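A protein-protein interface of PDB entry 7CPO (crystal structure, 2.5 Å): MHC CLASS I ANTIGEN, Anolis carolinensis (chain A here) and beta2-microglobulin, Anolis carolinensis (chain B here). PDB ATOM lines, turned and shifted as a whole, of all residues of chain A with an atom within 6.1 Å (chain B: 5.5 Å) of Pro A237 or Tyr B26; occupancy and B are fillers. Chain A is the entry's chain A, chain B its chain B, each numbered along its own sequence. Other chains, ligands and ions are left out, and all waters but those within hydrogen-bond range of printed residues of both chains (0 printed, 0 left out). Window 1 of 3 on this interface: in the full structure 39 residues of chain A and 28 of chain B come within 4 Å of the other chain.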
ATOM      1  N   LYS A 213       1.407 -22.788  -8.820  1.00  0.00           N
ATOM      2  CA  LYS A 213       1.777 -22.183 -10.097  1.00  0.00           C
ATOM      3  C   LYS A 213       0.563 -21.718 -10.908  1.00  0.00           C
ATOM      4  O   LYS A 213       0.662 -20.751 -11.674  1.00  0.00           O
ATOM      5  CB  LYS A 213       2.617 -23.189 -10.892  1.00  0.00           C
ATOM      6  CG  LYS A 213       3.685 -22.582 -11.784  1.00  0.00           C
ATOM      7  CD  LYS A 213       4.378 -23.623 -12.676  1.00  0.00           C
ATOM      8  CE  LYS A 213       5.457 -22.975 -13.581  1.00  0.00           C
ATOM      9  NZ  LYS A 213       5.905 -23.831 -14.734  1.00  0.00           N
ATOM     10  N   LEU A 234       7.189 -15.161 -19.132  1.00  0.00           N
ATOM     11  CA  LEU A 234       7.221 -16.517 -18.621  1.00  0.00           C
ATOM     12  C   LEU A 234       6.633 -16.561 -17.214  1.00  0.00           C
ATOM     13  O   LEU A 234       6.668 -15.578 -16.470  1.00  0.00           O
ATOM     14  CB  LEU A 234       8.658 -17.030 -18.592  1.00  0.00           C
ATOM     15  CG  LEU A 234       9.409 -16.914 -19.922  1.00  0.00           C
ATOM     16  CD1 LEU A 234      10.870 -17.196 -19.700  1.00  0.00           C
ATOM     17  CD2 LEU A 234       8.817 -17.840 -20.986  1.00  0.00           C
ATOM     18  N   VAL A 235       6.069 -17.707 -16.859  1.00  0.00           N
ATOM     19  CA  VAL A 235       5.762 -18.023 -15.471  1.00  0.00           C
ATOM     20  C   VAL A 235       7.024 -18.656 -14.901  1.00  0.00           C
ATOM     21  O   VAL A 235       7.367 -19.788 -15.248  1.00  0.00           O
ATOM     22  CB  VAL A 235       4.553 -18.960 -15.347  1.00  0.00           C
ATOM     23  CG1 VAL A 235       4.262 -19.236 -13.897  1.00  0.00           C
ATOM     24  CG2 VAL A 235       3.325 -18.352 -16.028  1.00  0.00           C
ATOM     25  N   SER A 236       7.727 -17.916 -14.047  1.00  0.00           N
ATOM     26  CA  SER A 236       9.083 -18.258 -13.672  1.00  0.00           C
ATOM     27  C   SER A 236       9.209 -18.403 -12.160  1.00  0.00           C
ATOM     28  O   SER A 236       8.535 -17.697 -11.394  1.00  0.00           O
ATOM     29  CB  SER A 236      10.072 -17.196 -14.170  1.00  0.00           C
ATOM     30  OG  SER A 236       9.721 -15.897 -13.707  1.00  0.00           O
ATOM     31  N   PRO A 237      10.071 -19.308 -11.705  1.00  0.00           N
ATOM     32  CA  PRO A 237      10.154 -19.593 -10.269  1.00  0.00           C
ATOM     33  C   PRO A 237      11.073 -18.644  -9.524  1.00  0.00           C
ATOM     34  O   PRO A 237      12.213 -18.401  -9.940  1.00  0.00           O
ATOM     35  CB  PRO A 237      10.718 -21.019 -10.237  1.00  0.00           C
ATOM     36  CG  PRO A 237      11.642 -21.039 -11.405  1.00  0.00           C
ATOM     37  CD  PRO A 237      10.968 -20.181 -12.481  1.00  0.00           C
ATOM     38  N   ASN A 238      10.576 -18.129  -8.407  1.00  0.00           N
ATOM     39  CA  ASN A 238      11.424 -17.515  -7.404  1.00  0.00           C
ATOM     40  C   ASN A 238      12.158 -18.589  -6.593  1.00  0.00           C
ATOM     41  O   ASN A 238      11.730 -19.747  -6.488  1.00  0.00           O
ATOM     42  CB  ASN A 238      10.588 -16.635  -6.475  1.00  0.00           C
ATOM     43  CG  ASN A 238       9.907 -15.488  -7.215  1.00  0.00           C
ATOM     44  OD1 ASN A 238       8.688 -15.358  -7.181  1.00  0.00           O
ATOM     45  ND2 ASN A 238      10.693 -14.653  -7.883  1.00  0.00           N
ATOM     46  N   SER A 239      13.280 -18.182  -6.004  1.00  0.00           N
ATOM     47  CA  SER A 239      14.080 -19.101  -5.215  1.00  0.00           C
ATOM     48  C   SER A 239      13.355 -19.592  -3.974  1.00  0.00           C
ATOM     49  O   SER A 239      13.730 -20.637  -3.437  1.00  0.00           O
ATOM     50  CB  SER A 239      15.377 -18.430  -4.795  1.00  0.00           C
ATOM     51  OG  SER A 239      15.097 -17.365  -3.901  1.00  0.00           O
ATOM     52  N   GLY A 241      10.454 -20.774  -3.963  1.00  0.00           N
ATOM     53  CA  GLY A 241       9.436 -21.678  -4.458  1.00  0.00           C
ATOM     54  C   GLY A 241       8.149 -21.026  -4.921  1.00  0.00           C
ATOM     55  O   GLY A 241       7.239 -21.733  -5.384  1.00  0.00           O
ATOM     56  N   THR A 242       8.040 -19.712  -4.818  1.00  0.00           N
ATOM     57  CA  THR A 242       6.876 -18.971  -5.267  1.00  0.00           C
ATOM     58  C   THR A 242       7.078 -18.638  -6.758  1.00  0.00           C
ATOM     59  O   THR A 242       8.149 -18.888  -7.316  1.00  0.00           O
ATOM     60  CB  THR A 242       6.734 -17.746  -4.348  1.00  0.00           C
ATOM     61  OG1 THR A 242       5.380 -17.326  -4.274  1.00  0.00           O
ATOM     62  CG2 THR A 242       7.573 -16.614  -4.829  1.00  0.00           C
ATOM     63  N   TYR A 243       6.053 -18.093  -7.430  1.00  0.00           N
ATOM     64  CA  TYR A 243       6.188 -17.821  -8.865  1.00  0.00           C
ATOM     65  C   TYR A 243       6.022 -16.346  -9.210  1.00  0.00           C
ATOM     66  O   TYR A 243       5.456 -15.558  -8.445  1.00  0.00           O
ATOM     67  CB  TYR A 243       5.194 -18.650  -9.693  1.00  0.00           C
ATOM     68  CG  TYR A 243       5.586 -20.101  -9.676  1.00  0.00           C
ATOM     69  CD1 TYR A 243       6.512 -20.603 -10.586  1.00  0.00           C
ATOM     70  CD2 TYR A 243       5.097 -20.949  -8.695  1.00  0.00           C
ATOM     71  CE1 TYR A 243       6.907 -21.912 -10.536  1.00  0.00           C
ATOM     72  CE2 TYR A 243       5.485 -22.247  -8.640  1.00  0.00           C
ATOM     73  CZ  TYR A 243       6.386 -22.735  -9.560  1.00  0.00           C
ATOM     74  OH  TYR A 243       6.751 -24.059  -9.475  1.00  0.00           O
ATOM     75  N   TYR A 244       6.509 -15.989 -10.403  1.00  0.00           N
ATOM     76  CA  TYR A 244       6.439 -14.619 -10.905  1.00  0.00           C
ATOM     77  C   TYR A 244       6.087 -14.611 -12.391  1.00  0.00           C
ATOM     78  O   TYR A 244       6.525 -15.491 -13.143  1.00  0.00           O
ATOM     79  CB  TYR A 244       7.776 -13.879 -10.693  1.00  0.00           C
ATOM     80  CG  TYR A 244       7.938 -12.623 -11.537  1.00  0.00           C
ATOM     81  CD1 TYR A 244       8.525 -12.684 -12.797  1.00  0.00           C
ATOM     82  CD2 TYR A 244       7.512 -11.373 -11.069  1.00  0.00           C
ATOM     83  CE1 TYR A 244       8.674 -11.558 -13.580  1.00  0.00           C
ATOM     84  CE2 TYR A 244       7.663 -10.230 -11.849  1.00  0.00           C
ATOM     85  CZ  TYR A 244       8.245 -10.336 -13.103  1.00  0.00           C
ATOM     86  OH  TYR A 244       8.420  -9.229 -13.898  1.00  0.00           O
ATOM     87  N   SER B   6      14.557 -19.127 -23.923  1.00  0.00           N
ATOM     88  CA  SER B   6      13.679 -18.041 -23.498  1.00  0.00           C
ATOM     89  C   SER B   6      14.070 -17.653 -22.079  1.00  0.00           C
ATOM     90  O   SER B   6      14.133 -18.514 -21.191  1.00  0.00           O
ATOM     91  CB  SER B   6      12.213 -18.470 -23.530  1.00  0.00           C
ATOM     92  OG  SER B   6      11.802 -18.738 -24.856  1.00  0.00           O
ATOM     93  N   VAL B   7      14.335 -16.368 -21.865  1.00  0.00           N
ATOM     94  CA  VAL B   7      14.994 -15.893 -20.655  1.00  0.00           C
ATOM     95  C   VAL B   7      14.147 -14.799 -20.016  1.00  0.00           C
ATOM     96  O   VAL B   7      13.418 -14.077 -20.700  1.00  0.00           O
ATOM     97  CB  VAL B   7      16.423 -15.402 -20.985  1.00  0.00           C
ATOM     98  CG1 VAL B   7      17.149 -14.819 -19.744  1.00  0.00           C
ATOM     99  CG2 VAL B   7      17.219 -16.536 -21.587  1.00  0.00           C
ATOM    100  N   GLN B   8      14.227 -14.696 -18.690  1.00  0.00           N
ATOM    101  CA  GLN B   8      13.465 -13.712 -17.938  1.00  0.00           C
ATOM    102  C   GLN B   8      14.237 -13.361 -16.672  1.00  0.00           C
ATOM    103  O   GLN B   8      14.796 -14.243 -16.016  1.00  0.00           O
ATOM    104  CB  GLN B   8      12.075 -14.251 -17.604  1.00  0.00           C
ATOM    105  CG  GLN B   8      11.203 -13.354 -16.777  1.00  0.00           C
ATOM    106  CD  GLN B   8       9.731 -13.568 -17.083  1.00  0.00           C
ATOM    107  OE1 GLN B   8       9.250 -13.177 -18.148  1.00  0.00           O
ATOM    108  NE2 GLN B   8       9.010 -14.199 -16.156  1.00  0.00           N
ATOM    109  N   VAL B   9      14.281 -12.075 -16.347  1.00  0.00           N
ATOM    110  CA  VAL B   9      14.962 -11.572 -15.160  1.00  0.00           C
ATOM    111  C   VAL B   9      13.950 -10.852 -14.278  1.00  0.00           C
ATOM    112  O   VAL B   9      13.026 -10.196 -14.774  1.00  0.00           O
ATOM    113  CB  VAL B   9      16.128 -10.634 -15.534  1.00  0.00           C
ATOM    114  CG1 VAL B   9      17.164 -11.383 -16.366  1.00  0.00           C
ATOM    115  CG2 VAL B   9      15.614  -9.387 -16.271  1.00  0.00           C
ATOM    116  N   TYR B  10      14.116 -10.980 -12.960  1.00  0.00           N
ATOM    117  CA  TYR B  10      13.134 -10.417 -12.036  1.00  0.00           C
ATOM    118  C   TYR B  10      13.704 -10.443 -10.623  1.00  0.00           C
ATOM    119  O   TYR B  10      14.636 -11.200 -10.330  1.00  0.00           O
ATOM    120  CB  TYR B  10      11.804 -11.185 -12.085  1.00  0.00           C
ATOM    121  CG  TYR B  10      11.989 -12.693 -12.011  1.00  0.00           C
ATOM    122  CD1 TYR B  10      11.793 -13.382 -10.817  1.00  0.00           C
ATOM    123  CD2 TYR B  10      12.385 -13.421 -13.133  1.00  0.00           C
ATOM    124  CE1 TYR B  10      11.983 -14.763 -10.746  1.00  0.00           C
ATOM    125  CE2 TYR B  10      12.590 -14.790 -13.069  1.00  0.00           C
ATOM    126  CZ  TYR B  10      12.379 -15.458 -11.879  1.00  0.00           C
ATOM    127  OH  TYR B  10      12.571 -16.819 -11.836  1.00  0.00           O
ATOM    128  N   HIS B  24      16.782 -12.825  -9.839  1.00  0.00           N
ATOM    129  CA  HIS B  24      16.709 -14.105 -10.531  1.00  0.00           C
ATOM    130  C   HIS B  24      16.945 -13.931 -12.020  1.00  0.00           C
ATOM    131  O   HIS B  24      16.503 -12.949 -12.617  1.00  0.00           O
ATOM    132  CB  HIS B  24      15.344 -14.785 -10.370  1.00  0.00           C
ATOM    133  CG  HIS B  24      14.869 -14.902  -8.954  1.00  0.00           C
ATOM    134  ND1 HIS B  24      14.345 -13.832  -8.255  1.00  0.00           N
ATOM    135  CD2 HIS B  24      14.787 -15.973  -8.126  1.00  0.00           C
ATOM    136  CE1 HIS B  24      13.982 -14.236  -7.048  1.00  0.00           C
ATOM    137  NE2 HIS B  24      14.238 -15.531  -6.944  1.00  0.00           N
ATOM    138  N   CYS B  25      17.600 -14.918 -12.622  1.00  0.00           N
ATOM    139  CA  CYS B  25      17.626 -15.075 -14.067  1.00  0.00           C
ATOM    140  C   CYS B  25      17.213 -16.506 -14.409  1.00  0.00           C
ATOM    141  O   CYS B  25      17.773 -17.470 -13.876  1.00  0.00           O
ATOM    142  CB  CYS B  25      19.006 -14.740 -14.638  1.00  0.00           C
ATOM    143  SG  CYS B  25      19.089 -14.940 -16.446  1.00  0.00           S
ATOM    144  N   TYR B  26      16.230 -16.641 -15.296  1.00  0.00           N
ATOM    145  CA  TYR B  26      15.588 -17.920 -15.564  1.00  0.00           C
ATOM    146  C   TYR B  26      15.559 -18.177 -17.063  1.00  0.00           C
ATOM    147  O   TYR B  26      15.127 -17.320 -17.838  1.00  0.00           O
ATOM    148  CB  TYR B  26      14.175 -17.944 -14.985  1.00  0.00           C
ATOM    149  CG  TYR B  26      13.431 -19.221 -15.248  1.00  0.00           C
ATOM    150  CD1 TYR B  26      13.833 -20.418 -14.668  1.00  0.00           C
ATOM    151  CD2 TYR B  26      12.318 -19.235 -16.078  1.00  0.00           C
ATOM    152  CE1 TYR B  26      13.140 -21.594 -14.912  1.00  0.00           C
ATOM    153  CE2 TYR B  26      11.631 -20.399 -16.327  1.00  0.00           C
ATOM    154  CZ  TYR B  26      12.046 -21.578 -15.744  1.00  0.00           C
ATOM    155  OH  TYR B  26      11.358 -22.743 -15.994  1.00  0.00           O
ATOM    156  N   ALA B  27      16.036 -19.346 -17.461  1.00  0.00           N
ATOM    157  CA  ALA B  27      16.105 -19.751 -18.851  1.00  0.00           C
ATOM    158  C   ALA B  27      15.339 -21.047 -19.018  1.00  0.00           C
ATOM    159  O   ALA B  27      15.401 -21.929 -18.159  1.00  0.00           O
ATOM    160  CB  ALA B  27      17.546 -19.948 -19.315  1.00  0.00           C
ATOM    161  N   GLU B  28      14.620 -21.164 -20.126  1.00  0.00           N
ATOM    162  CA  GLU B  28      13.828 -22.352 -20.377  1.00  0.00           C
ATOM    163  C   GLU B  28      13.715 -22.536 -21.882  1.00  0.00           C
ATOM    164  O   GLU B  28      14.106 -21.667 -22.663  1.00  0.00           O
ATOM    165  CB  GLU B  28      12.454 -22.256 -19.696  1.00  0.00           C
ATOM    166  CG  GLU B  28      11.468 -21.264 -20.311  1.00  0.00           C
ATOM    167  CD  GLU B  28      10.047 -21.487 -19.803  1.00  0.00           C
ATOM    168  OE1 GLU B  28       9.895 -22.194 -18.790  1.00  0.00           O
ATOM    169  OE2 GLU B  28       9.084 -20.960 -20.397  1.00  0.00           O
ATOM    170  N   LYS B  57      11.072 -30.168 -19.329  1.00  0.00           N
ATOM    171  CA  LYS B  57       9.634 -30.277 -19.481  1.00  0.00           C
ATOM    172  C   LYS B  57       9.294 -31.496 -20.315  1.00  0.00           C
ATOM    173  O   LYS B  57      10.170 -32.186 -20.854  1.00  0.00           O
ATOM    174  CB  LYS B  57       9.044 -29.029 -20.151  1.00  0.00           C
ATOM    175  CG  LYS B  57       9.311 -27.701 -19.456  1.00  0.00           C
ATOM    176  CD  LYS B  57       8.670 -26.544 -20.233  1.00  0.00           C
ATOM    177  CE  LYS B  57       9.445 -25.252 -20.012  1.00  0.00           C
ATOM    178  NZ  LYS B  57       9.294 -24.753 -18.621  1.00  0.00           N
ATOM    179  N   GLU B  63      15.449 -26.364 -18.290  1.00  0.00           N
ATOM    180  CA  GLU B  63      15.195 -25.185 -17.468  1.00  0.00           C
ATOM    181  C   GLU B  63      16.326 -25.025 -16.459  1.00  0.00           C
ATOM    182  O   GLU B  63      16.894 -26.009 -15.978  1.00  0.00           O
ATOM    183  CB  GLU B  63      13.872 -25.260 -16.685  1.00  0.00           C
ATOM    184  CG  GLU B  63      12.753 -25.999 -17.368  1.00  0.00           C
ATOM    185  CD  GLU B  63      11.611 -26.337 -16.417  1.00  0.00           C
ATOM    186  OE1 GLU B  63      11.890 -26.766 -15.268  1.00  0.00           O
ATOM    187  OE2 GLU B  63      10.437 -26.161 -16.819  1.00  0.00           O
ATOM    188  N   ARG B  64      16.622 -23.767 -16.114  1.00  0.00           N
ATOM    189  CA  ARG B  64      17.700 -23.449 -15.185  1.00  0.00           C
ATOM    190  C   ARG B  64      17.425 -22.099 -14.540  1.00  0.00           C
ATOM    191  O   ARG B  64      17.153 -21.115 -15.239  1.00  0.00           O
ATOM    192  CB  ARG B  64      19.055 -23.426 -15.899  1.00  0.00           C
ATOM    193  CG  ARG B  64      20.228 -23.006 -15.011  1.00  0.00           C
ATOM    194  CD  ARG B  64      20.709 -24.164 -14.153  1.00  0.00           C
ATOM    195  NE  ARG B  64      21.462 -25.132 -14.943  1.00  0.00           N
ATOM    196  CZ  ARG B  64      21.953 -26.266 -14.462  1.00  0.00           C
ATOM    197  NH1 ARG B  64      21.769 -26.579 -13.186  1.00  0.00           N
ATOM    198  NH2 ARG B  64      22.636 -27.081 -15.254  1.00  0.00           N
ATOM    199  N   LEU B  65      17.516 -22.054 -13.217  1.00  0.00           N
ATOM    200  CA  LEU B  65      17.308 -20.841 -12.445  1.00  0.00           C
ATOM    201  C   LEU B  65      18.612 -20.453 -11.759  1.00  0.00           C
ATOM    202  O   LEU B  65      19.329 -21.313 -11.238  1.00  0.00           O
ATOM    203  CB  LEU B  65      16.202 -21.032 -11.406  1.00  0.00           C
ATOM    204  CG  LEU B  65      15.967 -19.822 -10.501  1.00  0.00           C
ATOM    205  CD1 LEU B  65      15.333 -18.639 -11.265  1.00  0.00           C
ATOM    206  CD2 LEU B  65      15.116 -20.247  -9.329  1.00  0.00           C
ATOM    207  N   VAL B  66      18.921 -19.157 -11.782  1.00  0.00           N
ATOM    208  CA  VAL B  66      20.154 -18.600 -11.240  1.00  0.00           C
ATOM    209  C   VAL B  66      19.778 -17.367 -10.441  1.00  0.00           C
ATOM    210  O   VAL B  66      19.026 -16.517 -10.930  1.00  0.00           O
ATOM    211  CB  VAL B  66      21.153 -18.239 -12.353  1.00  0.00           C
ATOM    212  CG1 VAL B  66      22.451 -17.732 -11.757  1.00  0.00           C
ATOM    213  CG2 VAL B  66      21.421 -19.459 -13.253  1.00  0.00           C
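N of Tyr B26 lies within hydrogen-bond range of O of Gln B8. The backbone NH (N) of Ser B6 is in hydrogen-bond range of the backbone carbonyl oxygen (O) of Glu B28. O of Tyr A243 lies close to OD1 of Asn A238 (3.5 Å). N of Tyr A244 lies within hydrogen-bond range of O of Ser A236 (2.8 Å). OE1 of Glu B28 lies within salt-bridge range of NZ of Lys B57 (2.6 Å). The side-chain hydroxyl of Tyr B26 lies within hydrogen-bond range of the side-chain carboxylate of Glu B28 (3.2 Å).
Among the printed residues, merely in contact across the chains: Ser A236 with Tyr B10 (3.1 Å), Asn A238 with Tyr B10 (3.1 Å), Leu A234 with Glu B28 (3.2 Å), Pro A237 with Leu B65 (3.4 Å), Asn A238 with His B24 (3.4 Å), Tyr A244 with Tyr B10 (3.5 Å), Pro A237 with Tyr B26 (3.6 Å), Ser A236 with Tyr B26 (3.6 Å), Tyr A244 with Gln B8 (3.7 Å), Leu A234 with Ser B6 (3.8 Å) and Pro A237 with His B24 (3.98 Å).
Printed residues of chain B that touch a printed residue of chain A: Ser B6, Gln B8, Tyr B10, His B24, Tyr B26, Glu B28 and Leu B65. Hydrophobic or aromatic side chains of chain B within 4 Å of the printed part of chain A: Tyr B10, His B24, Tyr B26 and Leu B65.
Pro A237 touches four residues of chain B. Tyr B26 touches just these residues of chain A: Ser A236 and Pro A237. Printed residues of chain A within 4 Å of Ser B6: Leu A234. Of the printed residues of chain B, Ser A239 touches His B24. Of the printed residues of chain A, Tyr B10 touches Ser A236 (3.1 Å), Pro A237 (2.5 Å), Asn A238 (3.1 Å) and Tyr A244 (3.5 Å). Of the printed residues of chain A, Glu B28 touches Leu A234. Of the printed residues of chain A, His B24 touches Pro A237 (3.98 Å), Asn A238 (3.4 Å) and Ser A239 (3.0 Å). The nearest printed residue of chain B that does not touch Pro A237 is Arg B64 (6.7 Å). The nearest residue of chain A that does not touch Tyr B26 is Leu A234 (4.4 Å). The nearest printed residue of chain A that does not touch Glu B28 is Val A235 (5.0 Å).
The backbone carbonyl oxygen (O) of Leu A234 is in hydrogen-bond range of the side-chain amide nitrogen (NE2) of Gln B8, 2.7 Å away. The backbone NH (N) of Ser A239 sits at hydrogen-bond distance from a ring nitrogen (NE2) of His B24. OG of Ser A236 lies within hydrogen-bond range of NE2 of Gln B8. The backbone carbonyl oxygen (O) of Pro A237 lies within hydrogen-bond range of the side-chain hydroxyl (OH) of Tyr B10 (2.5 Å).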
